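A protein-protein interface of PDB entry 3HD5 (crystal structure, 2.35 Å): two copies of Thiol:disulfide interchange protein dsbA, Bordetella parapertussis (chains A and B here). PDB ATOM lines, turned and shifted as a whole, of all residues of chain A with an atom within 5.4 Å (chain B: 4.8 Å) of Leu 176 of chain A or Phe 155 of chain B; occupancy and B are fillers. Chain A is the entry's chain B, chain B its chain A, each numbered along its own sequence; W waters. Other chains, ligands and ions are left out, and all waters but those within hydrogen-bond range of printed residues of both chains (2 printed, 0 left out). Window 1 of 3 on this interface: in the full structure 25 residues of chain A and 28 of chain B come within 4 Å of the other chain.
SD of Met 46 of chain B lies within hydrogen-bond range of N of Ala 173 of chain A, 3.6 Å away.
The side-chain carboxylate of Asp 180 of chain A lies within hydrogen-bond range of the indole nitrogen of Trp 50 of chain B (2.8 Å).
The backbone carbonyl oxygen (O) of Thr 163 of chain B is in hydrogen-bond range of the backbone NH (N) of Phe 155 of chain B (2.7 Å).
Among the printed residues, merely in contact across the chains: Tyr 172 of chain A with Ile 43 of chain B, Tyr 172 of chain A with Met 46 of chain B, Tyr 172 of chain A with Pro 165 of chain B, Ala 175 of chain A with Pro 165 of chain B, Leu 176 of chain A with Met 46 of chain B, Leu 176 of chain A with Trp 50 of chain B, Leu 176 of chain A with Phe 155 of chain B, Val 178 of chain A with Thr 163 of chain B, Val 179 of chain A with Trp 50 of chain B, Val 179 of chain A with Phe 155 of chain B and Val 179 of chain A with Thr 163 of chain B.
Leu 176 of chain A touches just these residues of chain B: Met 46 (3.9 Å), Trp 50 (3.9 Å) and Phe 155 (3.9 Å).
Of chain A, only Leu 176 and Val 179 come within 4 Å of Phe 155 of chain B.
Printed residues of chain A within 4 Å of Pro 165 of chain B: Tyr 172 (3.8 Å) and Ala 175 (3.6 Å).
Of the printed residues of chain B, Asp 180 of chain A touches Trp 50 (2.8 Å).
The nearest printed residue of chain B that does not touch Val 179 of chain A is Val 157 of chain B (4.1 Å).
Of the 10 printed residues of chain A, 7 touch a printed residue of chain B.
Hydrophobic or aromatic side chains of chain A that line the printed part of chain B: Tyr 172, Ala 175, Leu 176, Val 178 and Val 179.
Among the printed residues, 13 pairs touch across the chains.
No position is printed for both chains.
Of the 13 pairs that touch across the chains among the printed residues, none has its exchanged pair printed and touching as well.
Water W1 lies within hydrogen-bond range of O of Ala 175 of chain A, OG1 of Thr 163 of chain B and O of Ser 164 of chain B.
Water W2 bridges O of Pro 165 of chain B and N of Ala 175 of chain A.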
ATOM      1  N   TYR A 172      31.710  -7.827   7.583  1.00  0.00           N
ATOM      2  CA  TYR A 172      31.388  -6.591   6.901  1.00  0.00           C
ATOM      3  C   TYR A 172      31.292  -6.780   5.396  1.00  0.00           C
ATOM      4  O   TYR A 172      30.508  -6.101   4.740  1.00  0.00           O
ATOM      5  CB  TYR A 172      32.391  -5.498   7.272  1.00  0.00           C
ATOM      6  CG  TYR A 172      32.273  -5.108   8.731  1.00  0.00           C
ATOM      7  CD1 TYR A 172      31.025  -5.039   9.350  1.00  0.00           C
ATOM      8  CD2 TYR A 172      33.403  -4.812   9.495  1.00  0.00           C
ATOM      9  CE1 TYR A 172      30.898  -4.689  10.697  1.00  0.00           C
ATOM     10  CE2 TYR A 172      33.288  -4.456  10.844  1.00  0.00           C
ATOM     11  CZ  TYR A 172      32.033  -4.402  11.434  1.00  0.00           C
ATOM     12  OH  TYR A 172      31.917  -4.085  12.762  1.00  0.00           O
ATOM     13  N   ALA A 173      32.061  -7.709   4.845  1.00  0.00           N
ATOM     14  CA  ALA A 173      31.995  -7.942   3.407  1.00  0.00           C
ATOM     15  C   ALA A 173      30.585  -8.412   3.036  1.00  0.00           C
ATOM     16  O   ALA A 173      30.061  -8.051   1.982  1.00  0.00           O
ATOM     17  CB  ALA A 173      33.013  -8.987   2.986  1.00  0.00           C
ATOM     18  N   GLY A 174      29.981  -9.214   3.911  1.00  0.00           N
ATOM     19  CA  GLY A 174      28.649  -9.723   3.650  1.00  0.00           C
ATOM     20  C   GLY A 174      27.630  -8.606   3.615  1.00  0.00           C
ATOM     21  O   GLY A 174      26.755  -8.556   2.748  1.00  0.00           O
ATOM     22  N   ALA A 175      27.756  -7.697   4.568  1.00  0.00           N
ATOM     23  CA  ALA A 175      26.854  -6.565   4.662  1.00  0.00           C
ATOM     24  C   ALA A 175      26.907  -5.755   3.374  1.00  0.00           C
ATOM     25  O   ALA A 175      25.884  -5.275   2.883  1.00  0.00           O
ATOM     26  CB  ALA A 175      27.245  -5.700   5.844  1.00  0.00           C
ATOM     27  N   LEU A 176      28.104  -5.606   2.819  1.00  0.00           N
ATOM     28  CA  LEU A 176      28.245  -4.839   1.590  1.00  0.00           C
ATOM     29  C   LEU A 176      27.713  -5.608   0.391  1.00  0.00           C
ATOM     30  O   LEU A 176      27.212  -5.010  -0.567  1.00  0.00           O
ATOM     31  CB  LEU A 176      29.706  -4.455   1.357  1.00  0.00           C
ATOM     32  CG  LEU A 176      30.264  -3.436   2.350  1.00  0.00           C
ATOM     33  CD1 LEU A 176      31.709  -3.137   2.001  1.00  0.00           C
ATOM     34  CD2 LEU A 176      29.421  -2.154   2.317  1.00  0.00           C
ATOM     35  N   LYS A 177      27.817  -6.931   0.431  1.00  0.00           N
ATOM     36  CA  LYS A 177      27.317  -7.702  -0.686  1.00  0.00           C
ATOM     37  C   LYS A 177      25.816  -7.449  -0.766  1.00  0.00           C
ATOM     38  O   LYS A 177      25.274  -7.275  -1.854  1.00  0.00           O
ATOM     39  CB  LYS A 177      27.598  -9.194  -0.515  1.00  0.00           C
ATOM     40  CG  LYS A 177      27.291  -9.967  -1.790  1.00  0.00           C
ATOM     41  CD  LYS A 177      27.471 -11.465  -1.644  1.00  0.00           C
ATOM     42  CE  LYS A 177      27.073 -12.172  -2.944  1.00  0.00           C
ATOM     43  NZ  LYS A 177      27.124 -13.657  -2.833  1.00  0.00           N
ATOM     44  N   VAL A 178      25.153  -7.421   0.389  1.00  0.00           N
ATOM     45  CA  VAL A 178      23.720  -7.151   0.428  1.00  0.00           C
ATOM     46  C   VAL A 178      23.465  -5.822  -0.272  1.00  0.00           C
ATOM     47  O   VAL A 178      22.555  -5.709  -1.092  1.00  0.00           O
ATOM     48  CB  VAL A 178      23.183  -7.047   1.875  1.00  0.00           C
ATOM     49  CG1 VAL A 178      21.791  -6.428   1.865  1.00  0.00           C
ATOM     50  CG2 VAL A 178      23.128  -8.429   2.517  1.00  0.00           C
ATOM     51  N   VAL A 179      24.284  -4.824   0.058  1.00  0.00           N
ATOM     52  CA  VAL A 179      24.169  -3.500  -0.544  1.00  0.00           C
ATOM     53  C   VAL A 179      24.254  -3.606  -2.068  1.00  0.00           C
ATOM     54  O   VAL A 179      23.491  -2.950  -2.780  1.00  0.00           O
ATOM     55  CB  VAL A 179      25.284  -2.535  -0.028  1.00  0.00           C
ATOM     56  CG1 VAL A 179      25.298  -1.258  -0.854  1.00  0.00           C
ATOM     57  CG2 VAL A 179      25.043  -2.189   1.430  1.00  0.00           C
ATOM     58  N   ASP A 180      25.175  -4.427  -2.570  1.00  0.00           N
ATOM     59  CA  ASP A 180      25.318  -4.583  -4.015  1.00  0.00           C
ATOM     60  C   ASP A 180      24.022  -5.099  -4.626  1.00  0.00           C
ATOM     61  O   ASP A 180      23.509  -4.538  -5.600  1.00  0.00           O
ATOM     62  CB  ASP A 180      26.458  -5.548  -4.357  1.00  0.00           C
ATOM     63  CG  ASP A 180      27.830  -4.978  -4.025  1.00  0.00           C
ATOM     64  OD1 ASP A 180      27.973  -3.739  -4.028  1.00  0.00           O
ATOM     65  OD2 ASP A 180      28.769  -5.765  -3.776  1.00  0.00           O
ATOM     66  N   GLN A 181      23.492  -6.163  -4.034  1.00  0.00           N
ATOM     67  CA  GLN A 181      22.262  -6.779  -4.505  1.00  0.00           C
ATOM     68  C   GLN A 181      21.085  -5.813  -4.392  1.00  0.00           C
ATOM     69  O   GLN A 181      20.190  -5.820  -5.237  1.00  0.00           O
ATOM     70  CB  GLN A 181      21.998  -8.066  -3.713  1.00  0.00           C
ATOM     71  CG  GLN A 181      23.137  -9.092  -3.854  1.00  0.00           C
ATOM     72  CD  GLN A 181      23.039 -10.263  -2.879  1.00  0.00           C
ATOM     73  OE1 GLN A 181      22.960 -10.074  -1.664  1.00  0.00           O
ATOM     74  NE2 GLN A 181      23.060 -11.482  -3.413  1.00  0.00           N
ATOM     75  N   VAL B  29      23.484   5.601  -2.198  1.00  0.00           N
ATOM     76  CA  VAL B  29      23.739   4.638  -1.139  1.00  0.00           C
ATOM     77  C   VAL B  29      24.187   5.526   0.005  1.00  0.00           C
ATOM     78  O   VAL B  29      25.227   6.184  -0.077  1.00  0.00           O
ATOM     79  CB  VAL B  29      24.876   3.654  -1.461  1.00  0.00           C
ATOM     80  CG1 VAL B  29      25.207   2.842  -0.207  1.00  0.00           C
ATOM     81  CG2 VAL B  29      24.465   2.725  -2.585  1.00  0.00           C
ATOM     82  N   LEU B  30      23.391   5.580   1.063  1.00  0.00           N
ATOM     83  CA  LEU B  30      23.755   6.413   2.195  1.00  0.00           C
ATOM     84  C   LEU B  30      24.266   5.556   3.344  1.00  0.00           C
ATOM     85  O   LEU B  30      23.599   4.599   3.760  1.00  0.00           O
ATOM     86  CB  LEU B  30      22.547   7.229   2.668  1.00  0.00           C
ATOM     87  CG  LEU B  30      21.792   8.059   1.625  1.00  0.00           C
ATOM     88  CD1 LEU B  30      20.721   8.866   2.328  1.00  0.00           C
ATOM     89  CD2 LEU B  30      22.739   8.986   0.901  1.00  0.00           C
ATOM     90  N   GLU B  31      25.455   5.893   3.844  1.00  0.00           N
ATOM     91  CA  GLU B  31      26.023   5.183   4.972  1.00  0.00           C
ATOM     92  C   GLU B  31      25.860   6.058   6.195  1.00  0.00           C
ATOM     93  O   GLU B  31      26.493   7.107   6.306  1.00  0.00           O
ATOM     94  CB  GLU B  31      27.521   4.895   4.790  1.00  0.00           C
ATOM     95  CG  GLU B  31      28.068   3.907   5.841  1.00  0.00           C
ATOM     96  CD  GLU B  31      29.516   4.169   6.283  1.00  0.00           C
ATOM     97  OE1 GLU B  31      30.317   4.730   5.506  1.00  0.00           O
ATOM     98  OE2 GLU B  31      29.858   3.791   7.427  1.00  0.00           O
ATOM     99  N   ILE B  43      34.731  -0.532   9.698  1.00  0.00           N
ATOM    100  CA  ILE B  43      34.268  -0.741   8.332  1.00  0.00           C
ATOM    101  C   ILE B  43      34.670   0.367   7.343  1.00  0.00           C
ATOM    102  O   ILE B  43      34.660   0.153   6.128  1.00  0.00           O
ATOM    103  CB  ILE B  43      32.717  -0.933   8.315  1.00  0.00           C
ATOM    104  CG1 ILE B  43      32.291  -1.761   7.098  1.00  0.00           C
ATOM    105  CG2 ILE B  43      32.013   0.428   8.287  1.00  0.00           C
ATOM    106  CD1 ILE B  43      30.789  -2.082   7.074  1.00  0.00           C
ATOM    107  N   MET B  46      36.849  -0.368   4.394  1.00  0.00           N
ATOM    108  CA  MET B  46      36.226  -1.307   3.472  1.00  0.00           C
ATOM    109  C   MET B  46      35.172  -0.566   2.644  1.00  0.00           C
ATOM    110  O   MET B  46      35.014  -0.819   1.452  1.00  0.00           O
ATOM    111  CB  MET B  46      35.583  -2.472   4.225  1.00  0.00           C
ATOM    112  CG  MET B  46      35.285  -3.676   3.327  1.00  0.00           C
ATOM    113  SD  MET B  46      34.539  -5.211   4.291  1.00  0.00           S
ATOM    114  CE  MET B  46      36.099  -5.644   5.370  1.00  0.00           C
ATOM    115  N   VAL B  47      34.457   0.354   3.277  1.00  0.00           N
ATOM    116  CA  VAL B  47      33.459   1.131   2.557  1.00  0.00           C
ATOM    117  C   VAL B  47      34.201   1.958   1.510  1.00  0.00           C
ATOM    118  O   VAL B  47      33.839   1.969   0.329  1.00  0.00           O
ATOM    119  CB  VAL B  47      32.698   2.091   3.492  1.00  0.00           C
ATOM    120  CG1 VAL B  47      31.723   2.943   2.686  1.00  0.00           C
ATOM    121  CG2 VAL B  47      31.952   1.300   4.560  1.00  0.00           C
ATOM    122  N   TRP B  50      35.246  -0.156  -1.221  1.00  0.00           N
ATOM    123  CA  TRP B  50      34.047  -0.568  -1.933  1.00  0.00           C
ATOM    124  C   TRP B  50      33.596   0.508  -2.916  1.00  0.00           C
ATOM    125  O   TRP B  50      33.233   0.208  -4.049  1.00  0.00           O
ATOM    126  CB  TRP B  50      32.909  -0.835  -0.944  1.00  0.00           C
ATOM    127  CG  TRP B  50      31.594  -1.115  -1.619  1.00  0.00           C
ATOM    128  CD1 TRP B  50      31.170  -2.311  -2.110  1.00  0.00           C
ATOM    129  CD2 TRP B  50      30.564  -0.165  -1.930  1.00  0.00           C
ATOM    130  NE1 TRP B  50      29.942  -2.172  -2.713  1.00  0.00           N
ATOM    131  CE2 TRP B  50      29.547  -0.863  -2.618  1.00  0.00           C
ATOM    132  CE3 TRP B  50      30.404   1.211  -1.696  1.00  0.00           C
ATOM    133  CZ2 TRP B  50      28.381  -0.235  -3.081  1.00  0.00           C
ATOM    134  CZ3 TRP B  50      29.243   1.838  -2.156  1.00  0.00           C
ATOM    135  CH2 TRP B  50      28.246   1.109  -2.843  1.00  0.00           C
ATOM    136  N   PRO B 153      27.002   0.773  11.904  1.00  0.00           N
ATOM    137  CA  PRO B 153      26.677   1.564  10.718  1.00  0.00           C
ATOM    138  C   PRO B 153      25.378   1.051  10.084  1.00  0.00           C
ATOM    139  O   PRO B 153      24.873  -0.012  10.449  1.00  0.00           O
ATOM    140  CB  PRO B 153      27.887   1.333   9.827  1.00  0.00           C
ATOM    141  CG  PRO B 153      28.180  -0.118  10.082  1.00  0.00           C
ATOM    142  CD  PRO B 153      28.059  -0.210  11.607  1.00  0.00           C
ATOM    143  N   ALA B 154      24.849   1.813   9.134  1.00  0.00           N
ATOM    144  CA  ALA B 154      23.622   1.440   8.452  1.00  0.00           C
ATOM    145  C   ALA B 154      23.607   2.005   7.036  1.00  0.00           C
ATOM    146  O   ALA B 154      24.091   3.113   6.788  1.00  0.00           O
ATOM    147  CB  ALA B 154      22.422   1.943   9.227  1.00  0.00           C
ATOM    148  N   PHE B 155      23.051   1.238   6.108  1.00  0.00           N
ATOM    149  CA  PHE B 155      22.992   1.672   4.730  1.00  0.00           C
ATOM    150  C   PHE B 155      21.568   1.778   4.192  1.00  0.00           C
ATOM    151  O   PHE B 155      20.728   0.903   4.421  1.00  0.00           O
ATOM    152  CB  PHE B 155      23.799   0.716   3.836  1.00  0.00           C
ATOM    153  CG  PHE B 155      25.238   0.537   4.265  1.00  0.00           C
ATOM    154  CD1 PHE B 155      25.571  -0.324   5.312  1.00  0.00           C
ATOM    155  CD2 PHE B 155      26.263   1.225   3.615  1.00  0.00           C
ATOM    156  CE1 PHE B 155      26.911  -0.499   5.705  1.00  0.00           C
ATOM    157  CE2 PHE B 155      27.605   1.059   3.999  1.00  0.00           C
ATOM    158  CZ  PHE B 155      27.927   0.194   5.046  1.00  0.00           C
ATOM    159  N   ALA B 156      21.307   2.873   3.487  1.00  0.00           N
ATOM    160  CA  ALA B 156      20.021   3.100   2.844  1.00  0.00           C
ATOM    161  C   ALA B 156      20.399   2.974   1.371  1.00  0.00           C
ATOM    162  O   ALA B 156      21.391   3.560   0.929  1.00  0.00           O
ATOM    163  CB  ALA B 156      19.499   4.503   3.151  1.00  0.00           C
ATOM    164  N   VAL B 157      19.631   2.199   0.617  1.00  0.00           N
ATOM    165  CA  VAL B 157      19.932   1.998  -0.793  1.00  0.00           C
ATOM    166  C   VAL B 157      18.759   2.366  -1.693  1.00  0.00           C
ATOM    167  O   VAL B 157      17.629   1.902  -1.493  1.00  0.00           O
ATOM    168  CB  VAL B 157      20.315   0.535  -1.061  1.00  0.00           C
ATOM    169  CG1 VAL B 157      20.661   0.357  -2.519  1.00  0.00           C
ATOM    170  CG2 VAL B 157      21.497   0.128  -0.173  1.00  0.00           C
ATOM    171  N   TYR B 161      15.619   0.716   0.512  1.00  0.00           N
ATOM    172  CA  TYR B 161      16.036  -0.268   1.505  1.00  0.00           C
ATOM    173  C   TYR B 161      17.043   0.189   2.549  1.00  0.00           C
ATOM    174  O   TYR B 161      17.864   1.087   2.328  1.00  0.00           O
ATOM    175  CB  TYR B 161      16.593  -1.498   0.791  1.00  0.00           C
ATOM    176  CG  TYR B 161      15.801  -1.870  -0.432  1.00  0.00           C
ATOM    177  CD1 TYR B 161      14.450  -2.189  -0.335  1.00  0.00           C
ATOM    178  CD2 TYR B 161      16.394  -1.879  -1.693  1.00  0.00           C
ATOM    179  CE1 TYR B 161      13.704  -2.508  -1.463  1.00  0.00           C
ATOM    180  CE2 TYR B 161      15.658  -2.197  -2.830  1.00  0.00           C
ATOM    181  CZ  TYR B 161      14.310  -2.510  -2.707  1.00  0.00           C
ATOM    182  OH  TYR B 161      13.563  -2.816  -3.825  1.00  0.00           O
ATOM    183  N   MET B 162      16.965  -0.458   3.698  1.00  0.00           N
ATOM    184  CA  MET B 162      17.865  -0.172   4.788  1.00  0.00           C
ATOM    185  C   MET B 162      18.482  -1.515   5.175  1.00  0.00           C
ATOM    186  O   MET B 162      17.773  -2.487   5.445  1.00  0.00           O
ATOM    187  CB  MET B 162      17.088   0.445   5.956  1.00  0.00           C
ATOM    188  CG  MET B 162      17.957   0.986   7.089  1.00  0.00           C
ATOM    189  SD  MET B 162      18.737  -0.388   8.231  1.00  0.00           S
ATOM    190  CE  MET B 162      17.375  -0.451   9.611  1.00  0.00           C
ATOM    191  N   THR B 163      19.804  -1.585   5.142  1.00  0.00           N
ATOM    192  CA  THR B 163      20.497  -2.802   5.526  1.00  0.00           C
ATOM    193  C   THR B 163      21.624  -2.405   6.471  1.00  0.00           C
ATOM    194  O   THR B 163      22.046  -1.242   6.492  1.00  0.00           O
ATOM    195  CB  THR B 163      21.079  -3.548   4.310  1.00  0.00           C
ATOM    196  OG1 THR B 163      21.577  -4.825   4.730  1.00  0.00           O
ATOM    197  CG2 THR B 163      22.197  -2.750   3.677  1.00  0.00           C
ATOM    198  N   SER B 164      22.087  -3.367   7.265  1.00  0.00           N
ATOM    199  CA  SER B 164      23.165  -3.137   8.218  1.00  0.00           C
ATOM    200  C   SER B 164      23.894  -4.456   8.412  1.00  0.00           C
ATOM    201  O   SER B 164      23.379  -5.513   8.045  1.00  0.00           O
ATOM    202  CB  SER B 164      22.603  -2.676   9.563  1.00  0.00           C
ATOM    203  OG  SER B 164      22.113  -3.783  10.298  1.00  0.00           O
ATOM    204  N   PRO B 165      25.113  -4.418   8.967  1.00  0.00           N
ATOM    205  CA  PRO B 165      25.805  -5.694   9.158  1.00  0.00           C
ATOM    206  C   PRO B 165      24.969  -6.639  10.007  1.00  0.00           C
ATOM    207  O   PRO B 165      24.858  -7.820   9.700  1.00  0.00           O
ATOM    208  CB  PRO B 165      27.104  -5.280   9.850  1.00  0.00           C
ATOM    209  CG  PRO B 165      27.396  -3.958   9.184  1.00  0.00           C
ATOM    210  CD  PRO B 165      26.028  -3.282   9.188  1.00  0.00           C
HETATM  211  O   HOH W   1      24.673  -4.408   5.145  1.00  0.00           O
HETATM  212  O   HOH W   2      27.388  -8.772   7.872  1.00  0.00           O
